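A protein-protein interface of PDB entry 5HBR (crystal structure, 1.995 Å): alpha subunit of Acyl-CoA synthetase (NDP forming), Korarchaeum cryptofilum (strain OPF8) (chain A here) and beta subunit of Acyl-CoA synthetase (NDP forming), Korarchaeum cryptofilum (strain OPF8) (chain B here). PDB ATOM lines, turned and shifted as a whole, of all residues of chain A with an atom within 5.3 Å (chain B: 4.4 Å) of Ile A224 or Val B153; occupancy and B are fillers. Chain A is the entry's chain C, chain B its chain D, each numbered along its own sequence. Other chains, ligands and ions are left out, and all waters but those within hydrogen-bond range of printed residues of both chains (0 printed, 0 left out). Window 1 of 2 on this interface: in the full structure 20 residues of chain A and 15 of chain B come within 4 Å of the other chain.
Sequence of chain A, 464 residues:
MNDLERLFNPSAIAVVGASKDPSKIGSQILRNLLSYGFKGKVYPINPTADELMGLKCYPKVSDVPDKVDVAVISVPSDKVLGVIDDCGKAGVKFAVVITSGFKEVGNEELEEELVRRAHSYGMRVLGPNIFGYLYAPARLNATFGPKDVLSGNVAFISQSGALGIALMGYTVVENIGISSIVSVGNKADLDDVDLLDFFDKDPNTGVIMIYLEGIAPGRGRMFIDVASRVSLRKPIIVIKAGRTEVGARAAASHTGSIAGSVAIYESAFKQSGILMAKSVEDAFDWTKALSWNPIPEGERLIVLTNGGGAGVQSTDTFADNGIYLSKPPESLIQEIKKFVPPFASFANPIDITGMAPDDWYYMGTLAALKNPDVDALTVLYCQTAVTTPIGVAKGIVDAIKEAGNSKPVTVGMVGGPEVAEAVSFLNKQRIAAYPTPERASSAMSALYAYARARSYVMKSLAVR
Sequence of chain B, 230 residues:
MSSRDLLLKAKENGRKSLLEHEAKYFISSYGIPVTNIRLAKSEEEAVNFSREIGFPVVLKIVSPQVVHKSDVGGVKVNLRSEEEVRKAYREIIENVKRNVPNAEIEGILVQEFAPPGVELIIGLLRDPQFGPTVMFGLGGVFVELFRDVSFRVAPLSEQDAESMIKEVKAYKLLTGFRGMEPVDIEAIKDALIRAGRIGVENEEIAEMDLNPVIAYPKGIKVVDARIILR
The backbone carbonyl oxygen of Ala B154 lies within hydrogen-bond range of the guanidinium group of Arg A221 (3.0 Å).
The side-chain amide oxygen of Gln A271 lies within hydrogen-bond range of the backbone NH of Val B153 (2.7 Å).
N of Ala B154 sits at hydrogen-bond distance from O of Pro B132, 2.9 Å away.
NH2 of Arg A221 lies within salt-bridge range of OD1 of Asp A225, 2.8 Å away.
The side-chain hydroxyl (OG) of Ser A228 lies within hydrogen-bond range of the backbone carbonyl oxygen (O) of Gln A271 (3.1 Å).
The backbone carbonyl oxygen of Ala A268 is in hydrogen-bond range of the side-chain hydroxyl of Ser A272, at 2.7 Å.
The backbone carbonyl oxygen of Ile A224 sits at hydrogen-bond distance from the side-chain hydroxyl of Ser A228, 2.6 Å away.
Among the printed residues, merely in contact across the chains: Gly A220 with Phe B130 (3.4 Å), Arg A221 with Val B153 (3.7 Å), Arg A221 with Pro B155 (3.6 Å), Ile A224 with Phe B130 (3.9 Å), Ile A224 with Val B153 (3.7 Å), Ile A264 with Phe B130 (3.7 Å), Ala A268 with Phe B130 (3.3 Å) and Gln A271 with Arg B152 (3.4 Å).
Ile A224 touches just these residues of chain B: Phe B130 (3.9 Å) and Val B153 (3.7 Å).
Val B153 touches just these residues of chain A: Arg A221, Ile A224 and Gln A271.
Of the printed residues of chain B, Arg A221 touches Val B153, Ala B154 and Pro B155.
Of the printed residues of chain B, Gln A271 touches Arg B152 (3.4 Å) and Val B153 (2.7 Å).
Val A226 touches none of the printed residues of chain B.
The nearest printed residue of chain B that does not touch Ile A224 is Ala B154 (6.4 Å).
The nearest printed residue of chain B that does not touch Arg A221 is Phe B130 (4.2 Å).
Of the 8 printed residues of chain B, 5 touch a printed residue of chain A.
Hydrophobic or aromatic side chains of chain B within 4 Å of the printed part of chain A: Phe B130, Val B153 and Pro B155.
Hydrophobic or aromatic side chains of chain A that line the printed part of chain B: Ile A224, Ile A264 and Ala A268.
Among the printed residues, 10 pairs touch across the chains.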
ATOM      1  N   GLY A 220      24.493 -10.273 -10.686  1.00  0.00           N
ATOM      2  CA  GLY A 220      24.602  -9.232  -9.672  1.00  0.00           C
ATOM      3  C   GLY A 220      24.091  -9.582  -8.281  1.00  0.00           C
ATOM      4  O   GLY A 220      24.673  -9.181  -7.275  1.00  0.00           O
ATOM      5  N   ARG A 221      22.995 -10.325  -8.218  1.00  0.00           N
ATOM      6  CA  ARG A 221      22.441 -10.754  -6.941  1.00  0.00           C
ATOM      7  C   ARG A 221      23.463 -11.586  -6.177  1.00  0.00           C
ATOM      8  O   ARG A 221      23.734 -11.332  -4.992  1.00  0.00           O
ATOM      9  CB  ARG A 221      21.154 -11.555  -7.153  1.00  0.00           C
ATOM     10  CG  ARG A 221      20.439 -11.956  -5.873  1.00  0.00           C
ATOM     11  CD  ARG A 221      19.983 -10.743  -5.070  1.00  0.00           C
ATOM     12  NE  ARG A 221      20.726 -10.614  -3.823  1.00  0.00           N
ATOM     13  CZ  ARG A 221      20.539  -9.654  -2.915  1.00  0.00           C
ATOM     14  NH1 ARG A 221      19.619  -8.711  -3.087  1.00  0.00           N
ATOM     15  NH2 ARG A 221      21.282  -9.637  -1.818  1.00  0.00           N
ATOM     16  N   MET A 222      24.035 -12.566  -6.867  1.00  0.00           N
ATOM     17  CA  MET A 222      25.019 -13.456  -6.285  1.00  0.00           C
ATOM     18  C   MET A 222      26.237 -12.629  -5.850  1.00  0.00           C
ATOM     19  O   MET A 222      26.825 -12.876  -4.799  1.00  0.00           O
ATOM     20  CB  MET A 222      25.391 -14.548  -7.307  1.00  0.00           C
ATOM     21  CG  MET A 222      26.383 -15.590  -6.834  1.00  0.00           C
ATOM     22  SD  MET A 222      25.692 -16.803  -5.694  1.00  0.00           S
ATOM     23  CE  MET A 222      27.096 -17.914  -5.524  1.00  0.00           C
ATOM     24  N   PHE A 223      26.590 -11.624  -6.643  1.00  0.00           N
ATOM     25  CA  PHE A 223      27.677 -10.728  -6.295  1.00  0.00           C
ATOM     26  C   PHE A 223      27.446 -10.038  -4.949  1.00  0.00           C
ATOM     27  O   PHE A 223      28.335  -9.991  -4.102  1.00  0.00           O
ATOM     28  CB  PHE A 223      27.866  -9.674  -7.383  1.00  0.00           C
ATOM     29  CG  PHE A 223      29.006  -8.736  -7.118  1.00  0.00           C
ATOM     30  CD1 PHE A 223      28.835  -7.630  -6.303  1.00  0.00           C
ATOM     31  CD2 PHE A 223      30.249  -8.967  -7.671  1.00  0.00           C
ATOM     32  CE1 PHE A 223      29.882  -6.768  -6.052  1.00  0.00           C
ATOM     33  CE2 PHE A 223      31.305  -8.105  -7.422  1.00  0.00           C
ATOM     34  CZ  PHE A 223      31.116  -7.008  -6.609  1.00  0.00           C
ATOM     35  N   ILE A 224      26.249  -9.502  -4.758  1.00  0.00           N
ATOM     36  CA  ILE A 224      25.900  -8.850  -3.505  1.00  0.00           C
ATOM     37  C   ILE A 224      25.978  -9.836  -2.350  1.00  0.00           C
ATOM     38  O   ILE A 224      26.527  -9.513  -1.293  1.00  0.00           O
ATOM     39  CB  ILE A 224      24.480  -8.231  -3.552  1.00  0.00           C
ATOM     40  CG1 ILE A 224      24.457  -7.073  -4.546  1.00  0.00           C
ATOM     41  CG2 ILE A 224      24.026  -7.754  -2.160  1.00  0.00           C
ATOM     42  CD1 ILE A 224      23.062  -6.574  -4.864  1.00  0.00           C
ATOM     43  N   ASP A 225      25.411 -11.024  -2.548  1.00  0.00           N
ATOM     44  CA  ASP A 225      25.350 -12.047  -1.502  1.00  0.00           C
ATOM     45  C   ASP A 225      26.747 -12.440  -1.020  1.00  0.00           C
ATOM     46  O   ASP A 225      26.979 -12.585   0.180  1.00  0.00           O
ATOM     47  CB  ASP A 225      24.632 -13.304  -1.997  1.00  0.00           C
ATOM     48  CG  ASP A 225      23.131 -13.101  -2.231  1.00  0.00           C
ATOM     49  OD1 ASP A 225      22.492 -12.202  -1.619  1.00  0.00           O
ATOM     50  OD2 ASP A 225      22.594 -13.876  -3.043  1.00  0.00           O
ATOM     51  N   VAL A 226      27.662 -12.621  -1.969  1.00  0.00           N
ATOM     52  CA  VAL A 226      29.023 -13.048  -1.674  1.00  0.00           C
ATOM     53  C   VAL A 226      29.855 -11.906  -1.107  1.00  0.00           C
ATOM     54  O   VAL A 226      30.439 -12.062  -0.042  1.00  0.00           O
ATOM     55  CB  VAL A 226      29.700 -13.620  -2.932  1.00  0.00           C
ATOM     56  CG1 VAL A 226      31.179 -13.903  -2.693  1.00  0.00           C
ATOM     57  CG2 VAL A 226      28.973 -14.892  -3.364  1.00  0.00           C
ATOM     58  N   ALA A 227      29.891 -10.767  -1.803  1.00  0.00           N
ATOM     59  CA  ALA A 227      30.632  -9.599  -1.334  1.00  0.00           C
ATOM     60  C   ALA A 227      30.181  -9.189   0.058  1.00  0.00           C
ATOM     61  O   ALA A 227      31.013  -8.861   0.904  1.00  0.00           O
ATOM     62  CB  ALA A 227      30.476  -8.437  -2.300  1.00  0.00           C
ATOM     63  N   SER A 228      28.869  -9.211   0.294  1.00  0.00           N
ATOM     64  CA  SER A 228      28.288  -8.888   1.604  1.00  0.00           C
ATOM     65  C   SER A 228      28.937  -9.665   2.752  1.00  0.00           C
ATOM     66  O   SER A 228      29.337  -9.101   3.769  1.00  0.00           O
ATOM     67  CB  SER A 228      26.775  -9.199   1.632  1.00  0.00           C
ATOM     68  OG  SER A 228      26.034  -8.217   0.949  1.00  0.00           O
ATOM     69  N   ARG A 229      29.002 -10.981   2.594  1.00  0.00           N
ATOM     70  CA  ARG A 229      29.547 -11.809   3.651  1.00  0.00           C
ATOM     71  C   ARG A 229      31.060 -11.623   3.766  1.00  0.00           C
ATOM     72  O   ARG A 229      31.592 -11.646   4.868  1.00  0.00           O
ATOM     73  CB  ARG A 229      29.192 -13.283   3.426  1.00  0.00           C
ATOM     74  CG  ARG A 229      29.951 -14.008   2.329  1.00  0.00           C
ATOM     75  CD  ARG A 229      30.067 -15.492   2.687  1.00  0.00           C
ATOM     76  NE  ARG A 229      30.491 -16.332   1.566  1.00  0.00           N
ATOM     77  CZ  ARG A 229      29.671 -16.814   0.638  1.00  0.00           C
ATOM     78  NH1 ARG A 229      28.376 -16.533   0.675  1.00  0.00           N
ATOM     79  NH2 ARG A 229      30.148 -17.584  -0.337  1.00  0.00           N
ATOM     80  N   ILE A 264      22.410   1.977  -9.992  1.00  0.00           N
ATOM     81  CA  ILE A 264      22.103   0.689  -9.387  1.00  0.00           C
ATOM     82  C   ILE A 264      23.396  -0.026  -8.956  1.00  0.00           C
ATOM     83  O   ILE A 264      23.441  -0.653  -7.891  1.00  0.00           O
ATOM     84  CB  ILE A 264      21.259  -0.162 -10.333  1.00  0.00           C
ATOM     85  CG1 ILE A 264      19.877   0.501 -10.492  1.00  0.00           C
ATOM     86  CG2 ILE A 264      21.065  -1.555  -9.789  1.00  0.00           C
ATOM     87  CD1 ILE A 264      19.066  -0.007 -11.687  1.00  0.00           C
ATOM     88  N   SER A 267      24.209   1.411  -5.604  1.00  0.00           N
ATOM     89  CA  SER A 267      23.406   0.862  -4.515  1.00  0.00           C
ATOM     90  C   SER A 267      23.830  -0.551  -4.172  1.00  0.00           C
ATOM     91  O   SER A 267      23.881  -0.919  -2.991  1.00  0.00           O
ATOM     92  CB  SER A 267      21.932   0.883  -4.864  1.00  0.00           C
ATOM     93  OG  SER A 267      21.573   2.193  -5.234  1.00  0.00           O
ATOM     94  N   ALA A 268      24.121  -1.341  -5.200  1.00  0.00           N
ATOM     95  CA  ALA A 268      24.622  -2.690  -5.001  1.00  0.00           C
ATOM     96  C   ALA A 268      25.922  -2.688  -4.205  1.00  0.00           C
ATOM     97  O   ALA A 268      26.145  -3.545  -3.343  1.00  0.00           O
ATOM     98  CB  ALA A 268      24.828  -3.367  -6.313  1.00  0.00           C
ATOM     99  N   GLN A 271      24.949  -2.037  -0.625  1.00  0.00           N
ATOM    100  CA  GLN A 271      24.341  -3.217  -0.006  1.00  0.00           C
ATOM    101  C   GLN A 271      25.381  -4.322   0.256  1.00  0.00           C
ATOM    102  O   GLN A 271      25.170  -5.193   1.094  1.00  0.00           O
ATOM    103  CB  GLN A 271      23.204  -3.753  -0.885  1.00  0.00           C
ATOM    104  CG  GLN A 271      21.999  -2.808  -0.973  1.00  0.00           C
ATOM    105  CD  GLN A 271      20.948  -3.280  -1.965  1.00  0.00           C
ATOM    106  OE1 GLN A 271      20.831  -2.736  -3.061  1.00  0.00           O
ATOM    107  NE2 GLN A 271      20.172  -4.279  -1.579  1.00  0.00           N
ATOM    108  N   SER A 272      26.509  -4.261  -0.452  1.00  0.00           N
ATOM    109  CA  SER A 272      27.583  -5.254  -0.317  1.00  0.00           C
ATOM    110  C   SER A 272      28.658  -4.856   0.686  1.00  0.00           C
ATOM    111  O   SER A 272      29.592  -5.621   0.918  1.00  0.00           O
ATOM    112  CB  SER A 272      28.248  -5.481  -1.663  1.00  0.00           C
ATOM    113  OG  SER A 272      27.313  -5.891  -2.638  1.00  0.00           O
ATOM    114  N   PHE B 130      21.372  -7.030 -11.822  1.00  0.00           N
ATOM    115  CA  PHE B 130      20.994  -7.238 -10.437  1.00  0.00           C
ATOM    116  C   PHE B 130      19.584  -7.767 -10.210  1.00  0.00           C
ATOM    117  O   PHE B 130      19.246  -8.170  -9.098  1.00  0.00           O
ATOM    118  CB  PHE B 130      21.202  -5.933  -9.691  1.00  0.00           C
ATOM    119  CG  PHE B 130      22.643  -5.540  -9.598  1.00  0.00           C
ATOM    120  CD1 PHE B 130      23.476  -6.149  -8.680  1.00  0.00           C
ATOM    121  CD2 PHE B 130      23.168  -4.585 -10.446  1.00  0.00           C
ATOM    122  CE1 PHE B 130      24.817  -5.799  -8.599  1.00  0.00           C
ATOM    123  CE2 PHE B 130      24.500  -4.234 -10.363  1.00  0.00           C
ATOM    124  CZ  PHE B 130      25.318  -4.845  -9.441  1.00  0.00           C
ATOM    125  N   PRO B 132      15.494  -7.883  -9.786  1.00  0.00           N
ATOM    126  CA  PRO B 132      14.471  -6.993  -9.241  1.00  0.00           C
ATOM    127  C   PRO B 132      15.073  -5.904  -8.338  1.00  0.00           C
ATOM    128  O   PRO B 132      15.812  -6.200  -7.403  1.00  0.00           O
ATOM    129  CB  PRO B 132      13.555  -7.944  -8.457  1.00  0.00           C
ATOM    130  CG  PRO B 132      14.390  -9.160  -8.206  1.00  0.00           C
ATOM    131  CD  PRO B 132      15.282  -9.282  -9.380  1.00  0.00           C
ATOM    132  N   THR B 133      14.760  -4.653  -8.662  1.00  0.00           N
ATOM    133  CA  THR B 133      15.274  -3.488  -7.957  1.00  0.00           C
ATOM    134  C   THR B 133      14.111  -2.569  -7.610  1.00  0.00           C
ATOM    135  O   THR B 133      13.235  -2.311  -8.442  1.00  0.00           O
ATOM    136  CB  THR B 133      16.321  -2.703  -8.805  1.00  0.00           C
ATOM    137  OG1 THR B 133      17.397  -3.567  -9.179  1.00  0.00           O
ATOM    138  CG2 THR B 133      16.890  -1.537  -8.018  1.00  0.00           C
ATOM    139  N   ARG B 152      17.437   0.156  -4.491  1.00  0.00           N
ATOM    140  CA  ARG B 152      17.951  -0.963  -3.706  1.00  0.00           C
ATOM    141  C   ARG B 152      17.612  -2.270  -4.412  1.00  0.00           C
ATOM    142  O   ARG B 152      16.480  -2.454  -4.870  1.00  0.00           O
ATOM    143  CB  ARG B 152      17.363  -0.953  -2.299  1.00  0.00           C
ATOM    144  CG  ARG B 152      17.910   0.142  -1.389  1.00  0.00           C
ATOM    145  CD  ARG B 152      19.396  -0.029  -1.108  1.00  0.00           C
ATOM    146  NE  ARG B 152      19.853   0.924  -0.097  1.00  0.00           N
ATOM    147  CZ  ARG B 152      20.123   2.205  -0.333  1.00  0.00           C
ATOM    148  NH1 ARG B 152      20.003   2.709  -1.550  1.00  0.00           N
ATOM    149  NH2 ARG B 152      20.518   2.987   0.657  1.00  0.00           N
ATOM    150  N   VAL B 153      18.584  -3.169  -4.509  1.00  0.00           N
ATOM    151  CA  VAL B 153      18.347  -4.471  -5.135  1.00  0.00           C
ATOM    152  C   VAL B 153      17.576  -5.345  -4.152  1.00  0.00           C
ATOM    153  O   VAL B 153      17.912  -5.405  -2.972  1.00  0.00           O
ATOM    154  CB  VAL B 153      19.674  -5.167  -5.566  1.00  0.00           C
ATOM    155  CG1 VAL B 153      19.382  -6.467  -6.301  1.00  0.00           C
ATOM    156  CG2 VAL B 153      20.478  -4.247  -6.458  1.00  0.00           C
ATOM    157  N   ALA B 154      16.533  -6.008  -4.641  1.00  0.00           N
ATOM    158  CA  ALA B 154      15.663  -6.837  -3.801  1.00  0.00           C
ATOM    159  C   ALA B 154      16.222  -8.236  -3.626  1.00  0.00           C
ATOM    160  O   ALA B 154      16.999  -8.694  -4.462  1.00  0.00           O
ATOM    161  CB  ALA B 154      14.234  -6.904  -4.418  1.00  0.00           C
ATOM    162  N   PRO B 155      15.831  -8.941  -2.543  1.00  0.00           N
ATOM    163  CA  PRO B 155      14.900  -8.528  -1.490  1.00  0.00           C
ATOM    164  C   PRO B 155      15.497  -7.462  -0.578  1.00  0.00           C
ATOM    165  O   PRO B 155      16.715  -7.437  -0.378  1.00  0.00           O
ATOM    166  CB  PRO B 155      14.663  -9.819  -0.717  1.00  0.00           C
ATOM    167  CG  PRO B 155      15.935 -10.538  -0.839  1.00  0.00           C
ATOM    168  CD  PRO B 155      16.423 -10.254  -2.236  1.00  0.00           C
ATOM    169  N   LEU B 156      14.638  -6.619  -0.021  1.00  0.00           N
ATOM    170  CA  LEU B 156      15.058  -5.514   0.833  1.00  0.00           C
ATOM    171  C   LEU B 156      14.990  -5.835   2.325  1.00  0.00           C
ATOM    172  O   LEU B 156      13.966  -6.287   2.823  1.00  0.00           O
ATOM    173  CB  LEU B 156      14.185  -4.292   0.567  1.00  0.00           C
ATOM    174  CG  LEU B 156      14.691  -3.278  -0.448  1.00  0.00           C
ATOM    175  CD1 LEU B 156      14.939  -3.947  -1.772  1.00  0.00           C
ATOM    176  CD2 LEU B 156      13.691  -2.160  -0.585  1.00  0.00           C
